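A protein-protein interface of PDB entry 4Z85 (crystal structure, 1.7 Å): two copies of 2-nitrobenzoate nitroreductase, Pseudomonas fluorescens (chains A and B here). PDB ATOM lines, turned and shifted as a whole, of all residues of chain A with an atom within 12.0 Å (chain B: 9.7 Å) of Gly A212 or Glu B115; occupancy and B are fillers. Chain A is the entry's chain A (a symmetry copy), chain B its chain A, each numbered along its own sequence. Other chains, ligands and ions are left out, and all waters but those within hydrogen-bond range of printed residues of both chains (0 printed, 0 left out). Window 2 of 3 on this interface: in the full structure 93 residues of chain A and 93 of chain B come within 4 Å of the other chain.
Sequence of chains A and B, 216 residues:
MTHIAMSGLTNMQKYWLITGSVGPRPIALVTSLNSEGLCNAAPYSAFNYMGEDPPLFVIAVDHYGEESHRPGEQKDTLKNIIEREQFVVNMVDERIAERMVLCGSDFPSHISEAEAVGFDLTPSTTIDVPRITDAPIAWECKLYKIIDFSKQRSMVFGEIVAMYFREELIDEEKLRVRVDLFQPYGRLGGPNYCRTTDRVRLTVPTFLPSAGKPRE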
ATOM      1  N   LEU A 208     -28.764 -20.382  30.260  1.00  0.00           N
ATOM      2  CA  LEU A 208     -28.521 -19.077  29.652  1.00  0.00           C
ATOM      3  C   LEU A 208     -28.153 -19.146  28.184  1.00  0.00           C
ATOM      4  O   LEU A 208     -27.305 -19.947  27.788  1.00  0.00           O
ATOM      5  CB  LEU A 208     -27.394 -18.341  30.387  1.00  0.00           C
ATOM      6  CG  LEU A 208     -27.535 -18.024  31.874  1.00  0.00           C
ATOM      7  CD1 LEU A 208     -26.230 -17.450  32.402  1.00  0.00           C
ATOM      8  CD2 LEU A 208     -28.672 -17.045  32.099  1.00  0.00           C
ATOM      9  N   PRO A 209     -28.759 -18.275  27.375  1.00  0.00           N
ATOM     10  CA  PRO A 209     -28.334 -18.112  25.988  1.00  0.00           C
ATOM     11  C   PRO A 209     -26.961 -17.470  25.901  1.00  0.00           C
ATOM     12  O   PRO A 209     -26.579 -16.674  26.766  1.00  0.00           O
ATOM     13  CB  PRO A 209     -29.398 -17.190  25.393  1.00  0.00           C
ATOM     14  CG  PRO A 209     -29.882 -16.406  26.532  1.00  0.00           C
ATOM     15  CD  PRO A 209     -29.818 -17.315  27.740  1.00  0.00           C
ATOM     16  N   SER A 210     -26.221 -17.843  24.870  1.00  0.00           N
ATOM     17  CA  SER A 210     -24.963 -17.193  24.548  1.00  0.00           C
ATOM     18  C   SER A 210     -24.821 -17.310  23.041  1.00  0.00           C
ATOM     19  O   SER A 210     -24.032 -18.114  22.538  1.00  0.00           O
ATOM     20  CB  SER A 210     -23.792 -17.834  25.294  1.00  0.00           C
ATOM     21  OG  SER A 210     -22.604 -17.074  25.131  1.00  0.00           O
ATOM     22  N   ALA A 211     -25.626 -16.531  22.322  1.00  0.00           N
ATOM     23  CA  ALA A 211     -25.705 -16.647  20.875  1.00  0.00           C
ATOM     24  C   ALA A 211     -24.469 -16.040  20.219  1.00  0.00           C
ATOM     25  O   ALA A 211     -23.985 -16.536  19.201  1.00  0.00           O
ATOM     26  CB  ALA A 211     -26.967 -15.978  20.356  1.00  0.00           C
ATOM     27  N   GLY A 212     -23.964 -14.962  20.809  1.00  0.00           N
ATOM     28  CA  GLY A 212     -22.764 -14.317  20.311  1.00  0.00           C
ATOM     29  C   GLY A 212     -21.541 -14.791  21.068  1.00  0.00           C
ATOM     30  O   GLY A 212     -20.432 -14.317  20.828  1.00  0.00           O
ATOM     31  N   THR B  31     -32.234  -0.481  27.000  1.00  0.00           N
ATOM     32  CA  THR B  31     -30.859  -0.624  26.527  1.00  0.00           C
ATOM     33  C   THR B  31     -30.012   0.527  27.071  1.00  0.00           C
ATOM     34  O   THR B  31     -30.464   1.684  27.146  1.00  0.00           O
ATOM     35  CB  THR B  31     -30.758  -0.680  24.981  1.00  0.00           C
ATOM     36  OG1 THR B  31     -31.573   0.329  24.376  1.00  0.00           O
ATOM     37  CG2 THR B  31     -31.186  -2.053  24.466  1.00  0.00           C
ATOM     38  N   GLY B  37     -18.555   0.700  26.021  1.00  0.00           N
ATOM     39  CA  GLY B  37     -19.412   0.798  24.850  1.00  0.00           C
ATOM     40  C   GLY B  37     -20.233  -0.460  24.629  1.00  0.00           C
ATOM     41  O   GLY B  37     -20.907  -0.605  23.607  1.00  0.00           O
ATOM     42  N   LEU B  38     -20.163  -1.373  25.592  1.00  0.00           N
ATOM     43  CA  LEU B  38     -20.955  -2.599  25.572  1.00  0.00           C
ATOM     44  C   LEU B  38     -22.419  -2.276  25.872  1.00  0.00           C
ATOM     45  O   LEU B  38     -22.706  -1.491  26.772  1.00  0.00           O
ATOM     46  CB  LEU B  38     -20.405  -3.600  26.591  1.00  0.00           C
ATOM     47  CG  LEU B  38     -20.910  -5.039  26.608  1.00  0.00           C
ATOM     48  CD1 LEU B  38     -19.960  -5.928  25.822  1.00  0.00           C
ATOM     49  CD2 LEU B  38     -21.043  -5.535  28.042  1.00  0.00           C
ATOM     50  N   CYS B  39     -23.339  -2.880  25.127  1.00  0.00           N
ATOM     51  CA  CYS B  39     -24.759  -2.593  25.326  1.00  0.00           C
ATOM     52  C   CYS B  39     -25.452  -3.640  26.191  1.00  0.00           C
ATOM     53  O   CYS B  39     -25.525  -4.819  25.831  1.00  0.00           O
ATOM     54  CB  CYS B  39     -25.481  -2.484  23.985  1.00  0.00           C
ATOM     55  SG  CYS B  39     -27.265  -2.047  24.131  1.00  0.00           S
ATOM     56  N   ASN B  40     -25.973  -3.197  27.329  1.00  0.00           N
ATOM     57  CA  ASN B  40     -26.759  -4.057  28.192  1.00  0.00           C
ATOM     58  C   ASN B  40     -28.239  -3.859  27.884  1.00  0.00           C
ATOM     59  O   ASN B  40     -28.647  -2.789  27.429  1.00  0.00           O
ATOM     60  CB  ASN B  40     -26.469  -3.766  29.663  1.00  0.00           C
ATOM     61  CG  ASN B  40     -25.075  -4.207  30.080  1.00  0.00           C
ATOM     62  OD1 ASN B  40     -24.242  -3.388  30.471  1.00  0.00           O
ATOM     63  ND2 ASN B  40     -24.823  -5.507  30.010  1.00  0.00           N
ATOM     64  N   ALA B  41     -29.022  -4.911  28.101  1.00  0.00           N
ATOM     65  CA  ALA B  41     -30.465  -4.856  27.879  1.00  0.00           C
ATOM     66  C   ALA B  41     -31.160  -5.561  29.031  1.00  0.00           C
ATOM     67  O   ALA B  41     -30.754  -6.653  29.427  1.00  0.00           O
ATOM     68  CB  ALA B  41     -30.829  -5.490  26.553  1.00  0.00           C
ATOM     69  N   ARG B  99     -36.994 -12.712  23.152  1.00  0.00           N
ATOM     70  CA  ARG B  99     -35.665 -12.221  23.464  1.00  0.00           C
ATOM     71  C   ARG B  99     -35.718 -11.279  24.663  1.00  0.00           C
ATOM     72  O   ARG B  99     -34.824 -11.281  25.507  1.00  0.00           O
ATOM     73  CB  ARG B  99     -35.056 -11.537  22.243  1.00  0.00           C
ATOM     74  CG  ARG B  99     -34.676 -12.519  21.139  1.00  0.00           C
ATOM     75  CD  ARG B  99     -34.231 -11.793  19.881  1.00  0.00           C
ATOM     76  NE  ARG B  99     -35.351 -11.215  19.149  1.00  0.00           N
ATOM     77  CZ  ARG B  99     -35.221 -10.410  18.102  1.00  0.00           C
ATOM     78  NH1 ARG B  99     -34.005 -10.084  17.654  1.00  0.00           N
ATOM     79  NH2 ARG B  99     -36.300  -9.918  17.506  1.00  0.00           N
ATOM     80  N   LEU B 102     -35.645 -13.472  27.563  1.00  0.00           N
ATOM     81  CA  LEU B 102     -34.276 -13.999  27.706  1.00  0.00           C
ATOM     82  C   LEU B 102     -33.333 -12.978  28.361  1.00  0.00           C
ATOM     83  O   LEU B 102     -32.434 -13.348  29.127  1.00  0.00           O
ATOM     84  CB  LEU B 102     -33.719 -14.432  26.350  1.00  0.00           C
ATOM     85  CG  LEU B 102     -34.472 -15.582  25.682  1.00  0.00           C
ATOM     86  CD1 LEU B 102     -33.843 -15.955  24.358  1.00  0.00           C
ATOM     87  CD2 LEU B 102     -34.545 -16.787  26.619  1.00  0.00           C
ATOM     88  N   CYS B 103     -33.557 -11.698  28.089  1.00  0.00           N
ATOM     89  CA  CYS B 103     -32.754 -10.635  28.700  1.00  0.00           C
ATOM     90  C   CYS B 103     -32.892 -10.550  30.207  1.00  0.00           C
ATOM     91  O   CYS B 103     -32.017 -10.010  30.885  1.00  0.00           O
ATOM     92  CB  CYS B 103     -33.124  -9.282  28.110  1.00  0.00           C
ATOM     93  SG  CYS B 103     -32.479  -9.004  26.498  1.00  0.00           S
ATOM     94  N   PHE B 107     -27.486 -13.275  33.925  1.00  0.00           N
ATOM     95  CA  PHE B 107     -26.189 -13.380  33.265  1.00  0.00           C
ATOM     96  C   PHE B 107     -25.050 -12.984  34.206  1.00  0.00           C
ATOM     97  O   PHE B 107     -23.920 -13.454  34.057  1.00  0.00           O
ATOM     98  CB  PHE B 107     -26.147 -12.513  32.004  1.00  0.00           C
ATOM     99  CG  PHE B 107     -27.108 -12.950  30.929  1.00  0.00           C
ATOM    100  CD1 PHE B 107     -26.737 -13.904  29.991  1.00  0.00           C
ATOM    101  CD2 PHE B 107     -28.379 -12.405  30.857  1.00  0.00           C
ATOM    102  CE1 PHE B 107     -27.618 -14.305  28.998  1.00  0.00           C
ATOM    103  CE2 PHE B 107     -29.261 -12.799  29.869  1.00  0.00           C
ATOM    104  CZ  PHE B 107     -28.885 -13.749  28.939  1.00  0.00           C
ATOM    105  N   ILE B 111     -21.950  -9.275  31.091  1.00  0.00           N
ATOM    106  CA  ILE B 111     -21.928  -9.536  29.656  1.00  0.00           C
ATOM    107  C   ILE B 111     -23.070  -8.802  28.954  1.00  0.00           C
ATOM    108  O   ILE B 111     -24.051  -8.413  29.588  1.00  0.00           O
ATOM    109  CB  ILE B 111     -22.010 -11.052  29.362  1.00  0.00           C
ATOM    110  CG1 ILE B 111     -23.361 -11.626  29.794  1.00  0.00           C
ATOM    111  CG2 ILE B 111     -20.891 -11.794  30.070  1.00  0.00           C
ATOM    112  CD1 ILE B 111     -24.358 -11.803  28.656  1.00  0.00           C
ATOM    113  N   SER B 112     -22.942  -8.613  27.646  1.00  0.00           N
ATOM    114  CA  SER B 112     -23.973  -7.928  26.882  1.00  0.00           C
ATOM    115  C   SER B 112     -25.150  -8.851  26.615  1.00  0.00           C
ATOM    116  O   SER B 112     -25.027  -9.814  25.861  1.00  0.00           O
ATOM    117  CB  SER B 112     -23.420  -7.410  25.557  1.00  0.00           C
ATOM    118  OG  SER B 112     -24.471  -7.149  24.639  1.00  0.00           O
ATOM    119  N   GLU B 113     -26.289  -8.554  27.229  1.00  0.00           N
ATOM    120  CA  GLU B 113     -27.487  -9.349  26.998  1.00  0.00           C
ATOM    121  C   GLU B 113     -27.896  -9.301  25.534  1.00  0.00           C
ATOM    122  O   GLU B 113     -28.352 -10.299  24.976  1.00  0.00           O
ATOM    123  CB  GLU B 113     -28.643  -8.867  27.876  1.00  0.00           C
ATOM    124  CG  GLU B 113     -28.439  -9.102  29.357  1.00  0.00           C
ATOM    125  CD  GLU B 113     -27.717  -7.949  30.045  1.00  0.00           C
ATOM    126  OE1 GLU B 113     -27.211  -7.043  29.342  1.00  0.00           O
ATOM    127  OE2 GLU B 113     -27.668  -7.953  31.292  1.00  0.00           O
ATOM    128  N   ALA B 114     -27.725  -8.138  24.915  1.00  0.00           N
ATOM    129  CA  ALA B 114     -28.168  -7.934  23.544  1.00  0.00           C
ATOM    130  C   ALA B 114     -27.451  -8.895  22.602  1.00  0.00           C
ATOM    131  O   ALA B 114     -28.032  -9.378  21.629  1.00  0.00           O
ATOM    132  CB  ALA B 114     -27.940  -6.499  23.127  1.00  0.00           C
ATOM    133  N   GLU B 115     -26.189  -9.175  22.911  1.00  0.00           N
ATOM    134  CA  GLU B 115     -25.397 -10.125  22.139  1.00  0.00           C
ATOM    135  C   GLU B 115     -25.794 -11.561  22.463  1.00  0.00           C
ATOM    136  O   GLU B 115     -25.950 -12.397  21.568  1.00  0.00           O
ATOM    137  CB  GLU B 115     -23.902  -9.924  22.409  1.00  0.00           C
ATOM    138  CG  GLU B 115     -23.042 -10.020  21.162  1.00  0.00           C
ATOM    139  CD  GLU B 115     -23.513  -9.076  20.071  1.00  0.00           C
ATOM    140  OE1 GLU B 115     -23.901  -7.933  20.402  1.00  0.00           O
ATOM    141  OE2 GLU B 115     -23.510  -9.477  18.886  1.00  0.00           O
ATOM    142  N   ALA B 116     -25.948 -11.840  23.753  1.00  0.00           N
ATOM    143  CA  ALA B 116     -26.265 -13.188  24.201  1.00  0.00           C
ATOM    144  C   ALA B 116     -27.613 -13.677  23.670  1.00  0.00           C
ATOM    145  O   ALA B 116     -27.778 -14.873  23.428  1.00  0.00           O
ATOM    146  CB  ALA B 116     -26.240 -13.257  25.722  1.00  0.00           C
ATOM    147  N   VAL B 117     -28.574 -12.770  23.486  1.00  0.00           N
ATOM    148  CA  VAL B 117     -29.930 -13.183  23.109  1.00  0.00           C
ATOM    149  C   VAL B 117     -30.265 -12.907  21.640  1.00  0.00           C
ATOM    150  O   VAL B 117     -31.314 -13.322  21.150  1.00  0.00           O
ATOM    151  CB  VAL B 117     -31.004 -12.501  24.005  1.00  0.00           C
ATOM    152  CG1 VAL B 117     -30.622 -12.612  25.473  1.00  0.00           C
ATOM    153  CG2 VAL B 117     -31.216 -11.041  23.603  1.00  0.00           C
ATOM    154  N   GLY B 118     -29.381 -12.216  20.930  1.00  0.00           N
ATOM    155  CA  GLY B 118     -29.580 -12.017  19.506  1.00  0.00           C
ATOM    156  C   GLY B 118     -30.373 -10.783  19.117  1.00  0.00           C
ATOM    157  O   GLY B 118     -31.142 -10.796  18.153  1.00  0.00           O
ATOM    158  N   PHE B 119     -30.195  -9.707  19.870  1.00  0.00           N
ATOM    159  CA  PHE B 119     -30.757  -8.426  19.477  1.00  0.00           C
ATOM    160  C   PHE B 119     -29.762  -7.669  18.603  1.00  0.00           C
ATOM    161  O   PHE B 119     -28.631  -7.432  19.022  1.00  0.00           O
ATOM    162  CB  PHE B 119     -31.091  -7.573  20.711  1.00  0.00           C
ATOM    163  CG  PHE B 119     -32.459  -7.822  21.289  1.00  0.00           C
ATOM    164  CD1 PHE B 119     -33.562  -7.968  20.466  1.00  0.00           C
ATOM    165  CD2 PHE B 119     -32.636  -7.885  22.662  1.00  0.00           C
ATOM    166  CE1 PHE B 119     -34.833  -8.168  21.008  1.00  0.00           C
ATOM    167  CE2 PHE B 119     -33.899  -8.103  23.211  1.00  0.00           C
ATOM    168  CZ  PHE B 119     -34.992  -8.237  22.379  1.00  0.00           C
ATOM    169  N   ASP B 120     -30.174  -7.270  17.408  1.00  0.00           N
ATOM    170  CA  ASP B 120     -29.383  -6.297  16.661  1.00  0.00           C
ATOM    171  C   ASP B 120     -29.697  -4.896  17.179  1.00  0.00           C
ATOM    172  O   ASP B 120     -30.790  -4.648  17.704  1.00  0.00           O
ATOM    173  CB  ASP B 120     -29.650  -6.391  15.160  1.00  0.00           C
ATOM    174  CG  ASP B 120     -29.049  -7.648  14.535  1.00  0.00           C
ATOM    175  OD1 ASP B 120     -27.882  -7.979  14.847  1.00  0.00           O
ATOM    176  OD2 ASP B 120     -29.744  -8.307  13.732  1.00  0.00           O
ATOM    177  N   LEU B 121     -28.733  -3.990  17.040  1.00  0.00           N
ATOM    178  CA  LEU B 121     -28.867  -2.636  17.563  1.00  0.00           C
ATOM    179  C   LEU B 121     -28.793  -1.594  16.455  1.00  0.00           C
ATOM    180  O   LEU B 121     -28.033  -1.736  15.491  1.00  0.00           O
ATOM    181  CB  LEU B 121     -27.792  -2.371  18.617  1.00  0.00           C
ATOM    182  CG  LEU B 121     -27.784  -3.362  19.779  1.00  0.00           C
ATOM    183  CD1 LEU B 121     -26.523  -3.220  20.607  1.00  0.00           C
ATOM    184  CD2 LEU B 121     -29.019  -3.140  20.652  1.00  0.00           C
ATOM    185  N   PRO B 130     -27.967   3.000  21.638  1.00  0.00           N
ATOM    186  CA  PRO B 130     -28.754   2.494  20.516  1.00  0.00           C
ATOM    187  C   PRO B 130     -30.056   1.840  20.974  1.00  0.00           C
ATOM    188  O   PRO B 130     -30.160   1.432  22.131  1.00  0.00           O
ATOM    189  CB  PRO B 130     -27.830   1.448  19.899  1.00  0.00           C
ATOM    190  CG  PRO B 130     -27.104   0.903  21.064  1.00  0.00           C
ATOM    191  CD  PRO B 130     -26.877   2.075  21.994  1.00  0.00           C
ATOM    192  N   ILE B 132     -33.047  -1.244  20.096  1.00  0.00           N
ATOM    193  CA  ILE B 132     -33.120  -2.590  19.542  1.00  0.00           C
ATOM    194  C   ILE B 132     -33.709  -2.512  18.143  1.00  0.00           C
ATOM    195  O   ILE B 132     -34.722  -1.850  17.931  1.00  0.00           O
ATOM    196  CB  ILE B 132     -33.961  -3.502  20.450  1.00  0.00           C
ATOM    197  CG1 ILE B 132     -33.155  -3.841  21.709  1.00  0.00           C
ATOM    198  CG2 ILE B 132     -34.405  -4.763  19.706  1.00  0.00           C
ATOM    199  CD1 ILE B 132     -33.978  -4.440  22.816  1.00  0.00           C
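Gly A212 touches just one residue of chain B: Glu B115.
Printed residues of chain A within 4 Å of Glu B115: Ala A211 and Gly A212.
Of chain B, only Ala B116 (3.7 Å) comes within 4 Å of Ser A210.
Ala A211 touches just these residues of chain B: Glu B115 (3.9 Å) and Ala B116 (2.9 Å).
No residue of chain A comes within 4 Å of Ser B112.
Ala B114 touches none of the printed residues of chain A.
Gly B118 touches none of the printed residues of chain A.
Of the printed residues of chain B, Pro A209 touches Phe B107 and Ala B116.
Of the printed residues of chain A, Phe B107 touches Pro A209.
Arg B99 touches none of the printed residues of chain A.
Leu A208 touches none of the printed residues of chain B.
The nearest residue of chain B that does not touch Gly A212 is Ala B116 (4.5 Å).
Hydrophobic or aromatic side chains of chain B within 4 Å of the printed part of chain A: Phe B107 and Ala B116.
Of the 5 printed residues of chain A, 4 touch a printed residue of chain B.
Printed residues of chain A that touch a printed residue of chain B: Pro A209, Ser A210, Ala A211 and Gly A212.
Hydrophobic or aromatic side chains of chain A within 4 Å of the printed part of chain B: Pro A209 and Ala A211.
Among the printed residues, no Asp or Glu carboxylate lies within 4 Å of a Lys or Arg side-chain nitrogen of the other chain.
Among the printed residues, merely in contact across the chains: Pro A209 with Phe B107, Pro A209 with Ala B116, Ser A210 with Ala B116 and Ala A211 with Glu B115.
The backbone carbonyl oxygen (O) of Glu B115 is in hydrogen-bond range of the backbone NH (N) of Gly A212 (3.3 Å).
N of Ala A211 sits at hydrogen-bond distance from O of Ala B116, at 2.9 Å.
The side-chain hydroxyl (OG) of Ser B112 sits at hydrogen-bond distance from the backbone NH (N) of Glu B115 (3.2 Å).
No position is printed for both chains.
Of the 6 pairs that touch across the chains among the printed residues, none has its exchanged pair printed and touching as well.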
